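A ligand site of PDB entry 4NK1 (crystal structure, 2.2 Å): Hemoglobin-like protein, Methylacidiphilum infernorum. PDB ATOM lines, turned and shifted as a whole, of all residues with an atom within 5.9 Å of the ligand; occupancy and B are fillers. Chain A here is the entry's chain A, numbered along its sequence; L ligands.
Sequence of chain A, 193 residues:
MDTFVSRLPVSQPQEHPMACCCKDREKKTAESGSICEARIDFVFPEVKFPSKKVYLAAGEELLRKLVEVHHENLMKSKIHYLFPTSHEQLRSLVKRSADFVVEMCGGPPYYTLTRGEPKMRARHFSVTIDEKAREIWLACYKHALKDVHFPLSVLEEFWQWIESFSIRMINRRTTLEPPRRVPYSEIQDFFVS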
ATOM      1  N   ILE A  79      33.331  -3.111  -8.814  1.00  0.00           N
ATOM      2  CA  ILE A  79      32.016  -2.544  -8.464  1.00  0.00           C
ATOM      3  C   ILE A  79      31.576  -1.471  -9.459  1.00  0.00           C
ATOM      4  O   ILE A  79      30.691  -0.676  -9.157  1.00  0.00           O
ATOM      5  CB  ILE A  79      31.945  -1.965  -7.019  1.00  0.00           C
ATOM      6  CG1 ILE A  79      32.877  -0.752  -6.850  1.00  0.00           C
ATOM      7  CG2 ILE A  79      32.274  -3.027  -5.977  1.00  0.00           C
ATOM      8  CD1 ILE A  79      32.924  -0.233  -5.415  1.00  0.00           C
ATOM      9  N   LEU A  82      27.800  -0.759 -10.217  1.00  0.00           N
ATOM     10  CA  LEU A  82      26.916   0.000  -9.322  1.00  0.00           C
ATOM     11  C   LEU A  82      26.746   1.459  -9.733  1.00  0.00           C
ATOM     12  O   LEU A  82      25.921   2.171  -9.161  1.00  0.00           O
ATOM     13  CB  LEU A  82      27.437  -0.042  -7.887  1.00  0.00           C
ATOM     14  CG  LEU A  82      27.479  -1.429  -7.247  1.00  0.00           C
ATOM     15  CD1 LEU A  82      28.215  -1.387  -5.919  1.00  0.00           C
ATOM     16  CD2 LEU A  82      26.056  -1.953  -7.073  1.00  0.00           C
ATOM     17  N   PHE A  83      27.514   1.897 -10.732  1.00  0.00           N
ATOM     18  CA  PHE A  83      27.583   3.306 -11.084  1.00  0.00           C
ATOM     19  C   PHE A  83      27.090   3.526 -12.485  1.00  0.00           C
ATOM     20  O   PHE A  83      27.236   2.652 -13.333  1.00  0.00           O
ATOM     21  CB  PHE A  83      29.039   3.793 -10.998  1.00  0.00           C
ATOM     22  CG  PHE A  83      29.597   3.748  -9.603  1.00  0.00           C
ATOM     23  CD1 PHE A  83      29.510   4.848  -8.774  1.00  0.00           C
ATOM     24  CD2 PHE A  83      30.164   2.579  -9.114  1.00  0.00           C
ATOM     25  CE1 PHE A  83      29.999   4.809  -7.488  1.00  0.00           C
ATOM     26  CE2 PHE A  83      30.666   2.526  -7.816  1.00  0.00           C
ATOM     27  CZ  PHE A  83      30.573   3.651  -7.001  1.00  0.00           C
ATOM     28  N   PRO A  84      26.543   4.735 -12.741  1.00  0.00           N
ATOM     29  CA  PRO A  84      26.136   5.093 -14.098  1.00  0.00           C
ATOM     30  C   PRO A  84      27.324   5.143 -15.053  1.00  0.00           C
ATOM     31  O   PRO A  84      28.488   5.209 -14.610  1.00  0.00           O
ATOM     32  CB  PRO A  84      25.577   6.518 -13.936  1.00  0.00           C
ATOM     33  CG  PRO A  84      25.469   6.769 -12.477  1.00  0.00           C
ATOM     34  CD  PRO A  84      26.462   5.872 -11.805  1.00  0.00           C
ATOM     35  N   GLN A  89      25.887  11.679 -16.494  1.00  0.00           N
ATOM     36  CA  GLN A  89      25.521  11.207 -15.157  1.00  0.00           C
ATOM     37  C   GLN A  89      26.719  11.043 -14.214  1.00  0.00           C
ATOM     38  O   GLN A  89      26.593  11.235 -13.004  1.00  0.00           O
ATOM     39  CB  GLN A  89      24.700   9.910 -15.210  1.00  0.00           C
ATOM     40  CG  GLN A  89      23.274  10.095 -15.761  1.00  0.00           C
ATOM     41  CD  GLN A  89      22.345   8.925 -15.408  1.00  0.00           C
ATOM     42  OE1 GLN A  89      21.464   9.066 -14.558  1.00  0.00           O
ATOM     43  NE2 GLN A  89      22.531   7.787 -16.074  1.00  0.00           N
ATOM     44  N   LEU A  93      27.409  12.900 -10.541  1.00  0.00           N
ATOM     45  CA  LEU A  93      27.844  12.157  -9.366  1.00  0.00           C
ATOM     46  C   LEU A  93      29.107  12.781  -8.800  1.00  0.00           C
ATOM     47  O   LEU A  93      29.165  13.151  -7.621  1.00  0.00           O
ATOM     48  CB  LEU A  93      28.139  10.719  -9.777  1.00  0.00           C
ATOM     49  CG  LEU A  93      28.043   9.576  -8.783  1.00  0.00           C
ATOM     50  CD1 LEU A  93      29.088   8.498  -9.076  1.00  0.00           C
ATOM     51  CD2 LEU A  93      28.133  10.041  -7.340  1.00  0.00           C
ATOM     52  N   ARG A  96      28.589  16.174  -7.131  1.00  0.00           N
ATOM     53  CA  ARG A  96      27.948  16.054  -5.821  1.00  0.00           C
ATOM     54  C   ARG A  96      28.887  15.453  -4.775  1.00  0.00           C
ATOM     55  O   ARG A  96      28.980  15.937  -3.638  1.00  0.00           O
ATOM     56  CB  ARG A  96      26.664  15.211  -5.907  1.00  0.00           C
ATOM     57  CG  ARG A  96      25.665  15.725  -6.935  1.00  0.00           C
ATOM     58  CD  ARG A  96      24.264  15.134  -6.745  1.00  0.00           C
ATOM     59  NE  ARG A  96      24.246  13.677  -6.694  1.00  0.00           N
ATOM     60  CZ  ARG A  96      24.167  12.880  -7.749  1.00  0.00           C
ATOM     61  NH1 ARG A  96      24.127  13.397  -8.976  1.00  0.00           N
ATOM     62  NH2 ARG A  96      24.141  11.556  -7.603  1.00  0.00           N
ATOM     63  N   SER A  97      29.558  14.380  -5.174  1.00  0.00           N
ATOM     64  CA  SER A  97      30.494  13.693  -4.285  1.00  0.00           C
ATOM     65  C   SER A  97      31.623  14.635  -3.887  1.00  0.00           C
ATOM     66  O   SER A  97      32.026  14.675  -2.715  1.00  0.00           O
ATOM     67  CB  SER A  97      31.060  12.468  -4.997  1.00  0.00           C
ATOM     68  OG  SER A  97      31.896  11.725  -4.146  1.00  0.00           O
ATOM     69  N   PHE A 100      30.564  17.258  -1.455  1.00  0.00           N
ATOM     70  CA  PHE A 100      30.513  16.721  -0.098  1.00  0.00           C
ATOM     71  C   PHE A 100      31.923  16.692   0.511  1.00  0.00           C
ATOM     72  O   PHE A 100      32.138  17.170   1.627  1.00  0.00           O
ATOM     73  CB  PHE A 100      29.876  15.335  -0.116  1.00  0.00           C
ATOM     74  CG  PHE A 100      29.764  14.688   1.258  1.00  0.00           C
ATOM     75  CD1 PHE A 100      28.822  15.140   2.171  1.00  0.00           C
ATOM     76  CD2 PHE A 100      30.584  13.626   1.600  1.00  0.00           C
ATOM     77  CE1 PHE A 100      28.715  14.546   3.427  1.00  0.00           C
ATOM     78  CE2 PHE A 100      30.467  13.015   2.872  1.00  0.00           C
ATOM     79  CZ  PHE A 100      29.532  13.479   3.783  1.00  0.00           C
ATOM     80  N   VAL A 101      32.875  16.123  -0.215  1.00  0.00           N
ATOM     81  CA  VAL A 101      34.257  16.043   0.269  1.00  0.00           C
ATOM     82  C   VAL A 101      34.857  17.419   0.584  1.00  0.00           C
ATOM     83  O   VAL A 101      35.501  17.594   1.641  1.00  0.00           O
ATOM     84  CB  VAL A 101      35.144  15.285  -0.709  1.00  0.00           C
ATOM     85  CG1 VAL A 101      36.597  15.286  -0.236  1.00  0.00           C
ATOM     86  CG2 VAL A 101      34.636  13.844  -0.842  1.00  0.00           C
ATOM     87  N   TYR A 111      27.734  21.211  -0.395  1.00  0.00           N
ATOM     88  CA  TYR A 111      26.818  20.057  -0.378  1.00  0.00           C
ATOM     89  C   TYR A 111      25.501  20.363   0.347  1.00  0.00           C
ATOM     90  O   TYR A 111      24.409  20.114  -0.185  1.00  0.00           O
ATOM     91  CB  TYR A 111      27.485  18.819   0.239  1.00  0.00           C
ATOM     92  CG  TYR A 111      26.653  17.556   0.106  1.00  0.00           C
ATOM     93  CD1 TYR A 111      26.727  16.767  -1.044  1.00  0.00           C
ATOM     94  CD2 TYR A 111      25.763  17.170   1.104  1.00  0.00           C
ATOM     95  CE1 TYR A 111      25.953  15.610  -1.181  1.00  0.00           C
ATOM     96  CE2 TYR A 111      24.980  16.009   0.964  1.00  0.00           C
ATOM     97  CZ  TYR A 111      25.083  15.247  -0.170  1.00  0.00           C
ATOM     98  OH  TYR A 111      24.319  14.118  -0.302  1.00  0.00           O
ATOM     99  N   ARG A 115      22.428  19.575  -1.812  1.00  0.00           N
ATOM    100  CA  ARG A 115      21.771  18.308  -1.543  1.00  0.00           C
ATOM    101  C   ARG A 115      21.113  18.295  -0.178  1.00  0.00           C
ATOM    102  O   ARG A 115      20.138  17.562   0.036  1.00  0.00           O
ATOM    103  CB  ARG A 115      22.766  17.148  -1.645  1.00  0.00           C
ATOM    104  CG  ARG A 115      23.530  17.121  -2.938  1.00  0.00           C
ATOM    105  CD  ARG A 115      22.617  16.852  -4.091  1.00  0.00           C
ATOM    106  NE  ARG A 115      22.058  15.517  -4.031  1.00  0.00           N
ATOM    107  CZ  ARG A 115      21.138  15.070  -4.870  1.00  0.00           C
ATOM    108  NH1 ARG A 115      20.663  15.861  -5.811  1.00  0.00           N
ATOM    109  NH2 ARG A 115      20.671  13.822  -4.753  1.00  0.00           N
ATOM    110  N   MET A 120      24.178  10.067   5.156  1.00  0.00           N
ATOM    111  CA  MET A 120      24.884   9.307   4.147  1.00  0.00           C
ATOM    112  C   MET A 120      24.550   7.812   4.138  1.00  0.00           C
ATOM    113  O   MET A 120      24.390   7.228   3.059  1.00  0.00           O
ATOM    114  CB  MET A 120      26.392   9.564   4.299  1.00  0.00           C
ATOM    115  CG  MET A 120      27.182   9.738   2.980  1.00  0.00           C
ATOM    116  SD  MET A 120      26.422  10.570   1.577  1.00  0.00           S
ATOM    117  CE  MET A 120      26.146  12.225   2.205  1.00  0.00           C
ATOM    118  N   ARG A 123      21.212   7.644   2.479  1.00  0.00           N
ATOM    119  CA  ARG A 123      21.236   7.857   1.031  1.00  0.00           C
ATOM    120  C   ARG A 123      21.768   6.622   0.294  1.00  0.00           C
ATOM    121  O   ARG A 123      21.425   6.404  -0.867  1.00  0.00           O
ATOM    122  CB  ARG A 123      22.072   9.074   0.658  1.00  0.00           C
ATOM    123  CG  ARG A 123      21.489  10.408   1.111  1.00  0.00           C
ATOM    124  CD  ARG A 123      22.405  11.529   0.652  1.00  0.00           C
ATOM    125  NE  ARG A 123      22.010  12.839   1.150  1.00  0.00           N
ATOM    126  CZ  ARG A 123      21.221  13.674   0.488  1.00  0.00           C
ATOM    127  NH1 ARG A 123      20.738  13.325  -0.701  1.00  0.00           N
ATOM    128  NH2 ARG A 123      20.913  14.866   1.009  1.00  0.00           N
ATOM    129  N   HIS A 124      22.608   5.832   0.951  1.00  0.00           N
ATOM    130  CA  HIS A 124      23.202   4.651   0.306  1.00  0.00           C
ATOM    131  C   HIS A 124      22.371   3.374   0.359  1.00  0.00           C
ATOM    132  O   HIS A 124      22.745   2.368  -0.257  1.00  0.00           O
ATOM    133  CB  HIS A 124      24.597   4.376   0.856  1.00  0.00           C
ATOM    134  CG  HIS A 124      25.603   5.373   0.387  1.00  0.00           C
ATOM    135  ND1 HIS A 124      25.718   6.631   0.951  1.00  0.00           N
ATOM    136  CD2 HIS A 124      26.500   5.346  -0.623  1.00  0.00           C
ATOM    137  CE1 HIS A 124      26.661   7.304   0.325  1.00  0.00           C
ATOM    138  NE2 HIS A 124      27.144   6.545  -0.629  1.00  0.00           N
ATOM    139  N   VAL A 127      21.751   1.703  -2.902  1.00  0.00           N
ATOM    140  CA  VAL A 127      22.789   0.941  -3.573  1.00  0.00           C
ATOM    141  C   VAL A 127      23.033  -0.271  -2.702  1.00  0.00           C
ATOM    142  O   VAL A 127      23.060  -0.161  -1.474  1.00  0.00           O
ATOM    143  CB  VAL A 127      24.094   1.744  -3.674  1.00  0.00           C
ATOM    144  CG1 VAL A 127      25.110   1.016  -4.527  1.00  0.00           C
ATOM    145  CG2 VAL A 127      23.834   3.103  -4.269  1.00  0.00           C
ATOM    146  N   THR A 128      23.199  -1.438  -3.306  1.00  0.00           N
ATOM    147  CA  THR A 128      23.497  -2.617  -2.505  1.00  0.00           C
ATOM    148  C   THR A 128      24.998  -2.680  -2.232  1.00  0.00           C
ATOM    149  O   THR A 128      25.813  -2.813  -3.166  1.00  0.00           O
ATOM    150  CB  THR A 128      23.004  -3.892  -3.170  1.00  0.00           C
ATOM    151  OG1 THR A 128      21.572  -3.812  -3.294  1.00  0.00           O
ATOM    152  CG2 THR A 128      23.383  -5.109  -2.324  1.00  0.00           C
ATOM    153  N   ILE A 129      25.365  -2.581  -0.959  1.00  0.00           N
ATOM    154  CA  ILE A 129      26.772  -2.465  -0.595  1.00  0.00           C
ATOM    155  C   ILE A 129      27.142  -3.522   0.418  1.00  0.00           C
ATOM    156  O   ILE A 129      26.734  -3.441   1.592  1.00  0.00           O
ATOM    157  CB  ILE A 129      27.079  -1.079   0.012  1.00  0.00           C
ATOM    158  CG1 ILE A 129      26.680   0.040  -0.959  1.00  0.00           C
ATOM    159  CG2 ILE A 129      28.571  -0.981   0.415  1.00  0.00           C
ATOM    160  CD1 ILE A 129      26.872   1.425  -0.411  1.00  0.00           C
ATOM    161  N   ALA A 133      32.465  -4.616  -1.357  1.00  0.00           N
ATOM    162  CA  ALA A 133      32.238  -3.365  -2.057  1.00  0.00           C
ATOM    163  C   ALA A 133      32.903  -2.205  -1.316  1.00  0.00           C
ATOM    164  O   ALA A 133      33.494  -1.320  -1.935  1.00  0.00           O
ATOM    165  CB  ALA A 133      30.753  -3.116  -2.233  1.00  0.00           C
ATOM    166  N   ARG A 134      32.810  -2.210   0.008  1.00  0.00           N
ATOM    167  CA  ARG A 134      33.474  -1.184   0.782  1.00  0.00           C
ATOM    168  C   ARG A 134      35.001  -1.269   0.622  1.00  0.00           C
ATOM    169  O   ARG A 134      35.682  -0.241   0.479  1.00  0.00           O
ATOM    170  CB  ARG A 134      33.112  -1.294   2.266  1.00  0.00           C
ATOM    171  CG  ARG A 134      34.225  -0.708   3.168  1.00  0.00           C
ATOM    172  CD  ARG A 134      33.765  -0.561   4.589  1.00  0.00           C
ATOM    173  NE  ARG A 134      34.802   0.001   5.439  1.00  0.00           N
ATOM    174  CZ  ARG A 134      35.766  -0.705   6.026  1.00  0.00           C
ATOM    175  NH1 ARG A 134      35.812  -2.027   5.848  1.00  0.00           N
ATOM    176  NH2 ARG A 134      36.670  -0.099   6.778  1.00  0.00           N
ATOM    177  N   TRP A 137      35.877  -0.025  -2.840  1.00  0.00           N
ATOM    178  CA  TRP A 137      35.706   1.417  -2.813  1.00  0.00           C
ATOM    179  C   TRP A 137      36.889   2.085  -2.090  1.00  0.00           C
ATOM    180  O   TRP A 137      37.444   3.083  -2.572  1.00  0.00           O
ATOM    181  CB  TRP A 137      34.356   1.741  -2.148  1.00  0.00           C
ATOM    182  CG  TRP A 137      33.947   3.195  -2.103  1.00  0.00           C
ATOM    183  CD1 TRP A 137      33.096   3.841  -2.956  1.00  0.00           C
ATOM    184  CD2 TRP A 137      34.361   4.184  -1.140  1.00  0.00           C
ATOM    185  NE1 TRP A 137      32.975   5.168  -2.589  1.00  0.00           N
ATOM    186  CE2 TRP A 137      33.737   5.393  -1.471  1.00  0.00           C
ATOM    187  CE3 TRP A 137      35.209   4.150  -0.022  1.00  0.00           C
ATOM    188  CZ2 TRP A 137      33.923   6.563  -0.737  1.00  0.00           C
ATOM    189  CZ3 TRP A 137      35.384   5.312   0.722  1.00  0.00           C
ATOM    190  CH2 TRP A 137      34.745   6.507   0.353  1.00  0.00           C
ATOM    191  N   TRP A 161      39.237   9.083   8.121  1.00  0.00           N
ATOM    192  CA  TRP A 161      37.865   9.509   7.962  1.00  0.00           C
ATOM    193  C   TRP A 161      37.066   8.558   7.088  1.00  0.00           C
ATOM    194  O   TRP A 161      36.042   8.040   7.522  1.00  0.00           O
ATOM    195  CB  TRP A 161      37.791  10.929   7.376  1.00  0.00           C
ATOM    196  CG  TRP A 161      36.376  11.314   7.057  1.00  0.00           C
ATOM    197  CD1 TRP A 161      35.292  11.178   7.874  1.00  0.00           C
ATOM    198  CD2 TRP A 161      35.890  11.909   5.847  1.00  0.00           C
ATOM    199  NE1 TRP A 161      34.168  11.649   7.245  1.00  0.00           N
ATOM    200  CE2 TRP A 161      34.502  12.103   5.996  1.00  0.00           C
ATOM    201  CE3 TRP A 161      36.500  12.307   4.653  1.00  0.00           C
ATOM    202  CZ2 TRP A 161      33.711  12.668   4.992  1.00  0.00           C
ATOM    203  CZ3 TRP A 161      35.724  12.864   3.649  1.00  0.00           C
ATOM    204  CH2 TRP A 161      34.334  13.040   3.828  1.00  0.00           C
ATOM    205  N   ILE A 162      37.511   8.333   5.849  1.00  0.00           N
ATOM    206  CA  ILE A 162      36.733   7.468   4.973  1.00  0.00           C
ATOM    207  C   ILE A 162      36.778   5.988   5.378  1.00  0.00           C
ATOM    208  O   ILE A 162      35.844   5.241   5.103  1.00  0.00           O
ATOM    209  CB  ILE A 162      37.124   7.594   3.484  1.00  0.00           C
ATOM    210  CG1 ILE A 162      38.616   7.308   3.272  1.00  0.00           C
ATOM    211  CG2 ILE A 162      36.733   8.966   2.926  1.00  0.00           C
ATOM    212  CD1 ILE A 162      38.996   7.227   1.771  1.00  0.00           C
ATOM    213  N   PHE A 165      34.098   5.876   8.267  1.00  0.00           N
ATOM    214  CA  PHE A 165      32.792   6.337   7.827  1.00  0.00           C
ATOM    215  C   PHE A 165      32.190   5.333   6.834  1.00  0.00           C
ATOM    216  O   PHE A 165      30.972   5.069   6.881  1.00  0.00           O
ATOM    217  CB  PHE A 165      32.897   7.735   7.208  1.00  0.00           C
ATOM    218  CG  PHE A 165      31.563   8.442   7.057  1.00  0.00           C
ATOM    219  CD1 PHE A 165      30.529   8.209   7.952  1.00  0.00           C
ATOM    220  CD2 PHE A 165      31.346   9.326   6.003  1.00  0.00           C
ATOM    221  CE1 PHE A 165      29.286   8.851   7.814  1.00  0.00           C
ATOM    222  CE2 PHE A 165      30.095   9.978   5.845  1.00  0.00           C
ATOM    223  CZ  PHE A 165      29.071   9.727   6.765  1.00  0.00           C
ATOM    224  N   SER A 166      33.014   4.750   5.966  1.00  0.00           N
ATOM    225  CA  SER A 166      32.518   3.793   4.971  1.00  0.00           C
ATOM    226  C   SER A 166      31.873   2.543   5.564  1.00  0.00           C
ATOM    227  O   SER A 166      31.024   1.932   4.926  1.00  0.00           O
ATOM    228  CB  SER A 166      33.635   3.375   4.001  1.00  0.00           C
ATOM    229  OG  SER A 166      34.699   2.733   4.684  1.00  0.00           O
ATOM    230  N   ILE A 167      32.285   2.159   6.766  1.00  0.00           N
ATOM    231  CA  ILE A 167      31.683   0.982   7.409  1.00  0.00           C
ATOM    232  C   ILE A 167      30.183   1.223   7.564  1.00  0.00           C
ATOM    233  O   ILE A 167      29.362   0.299   7.448  1.00  0.00           O
ATOM    234  CB  ILE A 167      32.340   0.680   8.760  1.00  0.00           C
ATOM    235  CG1 ILE A 167      33.830   0.390   8.561  1.00  0.00           C
ATOM    236  CG2 ILE A 167      31.677  -0.504   9.459  1.00  0.00           C
ATOM    237  CD1 ILE A 167      34.625   0.377   9.846  1.00  0.00           C
ATOM    238  N   MET A 169      28.224   2.579   5.557  1.00  0.00           N
ATOM    239  CA  MET A 169      27.473   2.490   4.301  1.00  0.00           C
ATOM    240  C   MET A 169      27.079   1.045   3.963  1.00  0.00           C
ATOM    241  O   MET A 169      26.188   0.813   3.142  1.00  0.00           O
ATOM    242  CB  MET A 169      28.285   3.059   3.137  1.00  0.00           C
ATOM    243  CG  MET A 169      28.776   4.476   3.319  1.00  0.00           C
ATOM    244  SD  MET A 169      27.463   5.585   3.870  1.00  0.00           S
ATOM    245  CE  MET A 169      28.203   6.212   5.369  1.00  0.00           C
ATOM    246  N   ILE A 170      27.758   0.077   4.579  1.00  0.00           N
ATOM    247  CA  ILE A 170      27.474  -1.330   4.306  1.00  0.00           C
ATOM    248  C   ILE A 170      26.027  -1.664   4.686  1.00  0.00           C
ATOM    249  O   ILE A 170      25.635  -1.528   5.846  1.00  0.00           O
ATOM    250  CB  ILE A 170      28.400  -2.266   5.129  1.00  0.00           C
ATOM    251  CG1 ILE A 170      29.855  -2.136   4.671  1.00  0.00           C
ATOM    252  CG2 ILE A 170      27.924  -3.722   5.019  1.00  0.00           C
ATOM    253  CD1 ILE A 170      30.883  -2.806   5.636  1.00  0.00           C
HETATM  254  C1  LIG L   1      26.676   8.408  -3.994  1.00  0.00           C
HETATM  255  C2  LIG L   1      28.595   3.920  -3.978  1.00  0.00           C
HETATM  256  C3  LIG L   1      30.702   4.882   0.317  1.00  0.00           C
HETATM  257  C4  LIG L   1      29.814   9.606  -0.417  1.00  0.00           C
HETATM  258  C5  LIG L   1      26.955   7.088  -4.332  1.00  0.00           C
HETATM  259  C6  LIG L   1      26.366   6.354  -5.433  1.00  0.00           C
HETATM  260  C7  LIG L   1      26.882   5.110  -5.418  1.00  0.00           C
HETATM  261  C8  LIG L   1      27.842   5.018  -4.327  1.00  0.00           C
HETATM  262  C9  LIG L   1      26.565   3.965  -6.409  1.00  0.00           C
HETATM  263  C10 LIG L   1      25.290   6.928  -6.405  1.00  0.00           C
HETATM  264  C11 LIG L   1      25.815   7.087  -7.828  1.00  0.00           C
HETATM  265  C12 LIG L   1      24.940   8.051  -8.601  1.00  0.00           C
HETATM  266  O1  LIG L   1      24.043   8.679  -7.981  1.00  0.00           O
HETATM  267  O2  LIG L   1      25.124   8.223  -9.830  1.00  0.00           O
HETATM  268  C13 LIG L   1      29.284   3.748  -2.786  1.00  0.00           C
HETATM  269  C14 LIG L   1      29.885   2.520  -2.291  1.00  0.00           C
HETATM  270  C15 LIG L   1      30.452   2.781  -1.107  1.00  0.00           C
HETATM  271  C16 LIG L   1      30.262   4.192  -0.811  1.00  0.00           C
HETATM  272  C17 LIG L   1      29.863   1.143  -2.985  1.00  0.00           C
HETATM  273  C18 LIG L   1      31.197   1.732  -0.243  1.00  0.00           C
HETATM  274  C19 LIG L   1      31.415   1.904   1.079  1.00  0.00           C
HETATM  275  C20 LIG L   1      30.696   6.243   0.463  1.00  0.00           C
HETATM  276  C21 LIG L   1      31.361   7.000   1.509  1.00  0.00           C
HETATM  277  C22 LIG L   1      31.141   8.305   1.306  1.00  0.00           C
HETATM  278  C23 LIG L   1      30.297   8.434   0.126  1.00  0.00           C
HETATM  279  C24 LIG L   1      32.218   6.459   2.656  1.00  0.00           C
HETATM  280  C25 LIG L   1      31.701   9.418   2.218  1.00  0.00           C
HETATM  281  C26 LIG L   1      32.194  10.543   1.698  1.00  0.00           C
HETATM  282  C27 LIG L   1      28.834   9.735  -1.391  1.00  0.00           C
HETATM  283  C28 LIG L   1      28.151  10.958  -1.733  1.00  0.00           C
HETATM  284  C29 LIG L   1      27.161  10.585  -2.832  1.00  0.00           C
HETATM  285  C30 LIG L   1      27.356   9.178  -3.079  1.00  0.00           C
HETATM  286  C31 LIG L   1      28.335  12.358  -1.111  1.00  0.00           C
HETATM  287  C32 LIG L   1      26.187  11.565  -3.531  1.00  0.00           C
HETATM  288  C33 LIG L   1      24.869  11.566  -2.724  1.00  0.00           C
HETATM  289  C34 LIG L   1      23.927  12.606  -3.287  1.00  0.00           C
HETATM  290  O3  LIG L   1      23.421  12.401  -4.417  1.00  0.00           O
HETATM  291  O4  LIG L   1      23.694  13.647  -2.627  1.00  0.00           O
HETATM  292  N1  LIG L   1      27.844   6.244  -3.687  1.00  0.00           N
HETATM  293  N2  LIG L   1      29.545   4.751  -1.859  1.00  0.00           N
HETATM  294  N3  LIG L   1      30.040   7.153  -0.356  1.00  0.00           N
HETATM  295  N4  LIG L   1      28.338   8.716  -2.202  1.00  0.00           N
HETATM  296 FE1  LIG L   1      28.903   6.756  -2.048  1.00  0.00          FE
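An iron atom (FE1) of the ligand is bound by a ring nitrogen (NE2) of His 124, 2.3 Å away. O4 of the ligand lies within hydrogen-bond range of OH of Tyr 111 (2.5 Å). NE of Arg 115 is in salt-bridge range of O4 of the ligand, 2.9 Å away. NE of Arg 96 lies within salt-bridge range of O3 of the ligand. NH1 of Arg 123 lies within salt-bridge range of O4 of the ligand.
The guanidinium group (NE) of Arg 134 sits at hydrogen-bond distance from the side-chain hydroxyl (OG) of Ser 166 (2.8 Å). A ring nitrogen (ND1) of His 124 lies within hydrogen-bond range of the backbone carbonyl oxygen (O) of Met 120, at 2.6 Å. OH of Tyr 111 lies within hydrogen-bond range of NE of Arg 123, 3.0 Å away. A ring nitrogen (ND1) of His 124 lies within hydrogen-bond range of the side-chain sulfur of Met 169 (3.6 Å). The side-chain hydroxyl (OG) of Ser 166 lies within hydrogen-bond range of the backbone carbonyl oxygen (O) of Ile 162 (2.8 Å). NH2 of Arg 123 is in hydrogen-bond range of O of Arg 115, 3.0 Å away.
Leu 82 touches the ligand. Phe 83 touches the ligand. Pro 84 touches the ligand (CG to O2, 3.0 Å). Leu 93 touches the ligand. Phe 100 touches the ligand (CE2 to C26, 3.2 Å). Met 120 touches the ligand (SD to C31, 3.8 Å). CG2 of Val 127 touches C9 of the ligand, at 3.6 Å. Ile 129 touches the ligand (CD1 to C14, 3.7 Å). Arg 134 touches the ligand (CA to C19, 3.7 Å). Trp 137 touches the ligand (NE1 to C16, 3.4 Å). Trp 161 touches the ligand. Phe 165 touches the ligand. CA of Ser 166 touches C24 of the ligand, 3.5 Å away. Met 169 touches the ligand. Hydrophobic or aromatic side chains that line the ligand: Phe 83, Pro 84, Leu 93, Phe 100, Tyr 111, Met 120, His 124, Val 127, Ile 129, Trp 137, Trp 161, Phe 165 and Met 169. 19 residues have an atom within 4 Å of the ligand: Leu 82, Phe 83, Pro 84, Leu 93, Arg 96, Phe 100, Tyr 111, Arg 115, Met 120, Arg 123, His 124, Val 127, Ile 129, Arg 134, Trp 137, Trp 161, Phe 165, Ser 166 and Met 169.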
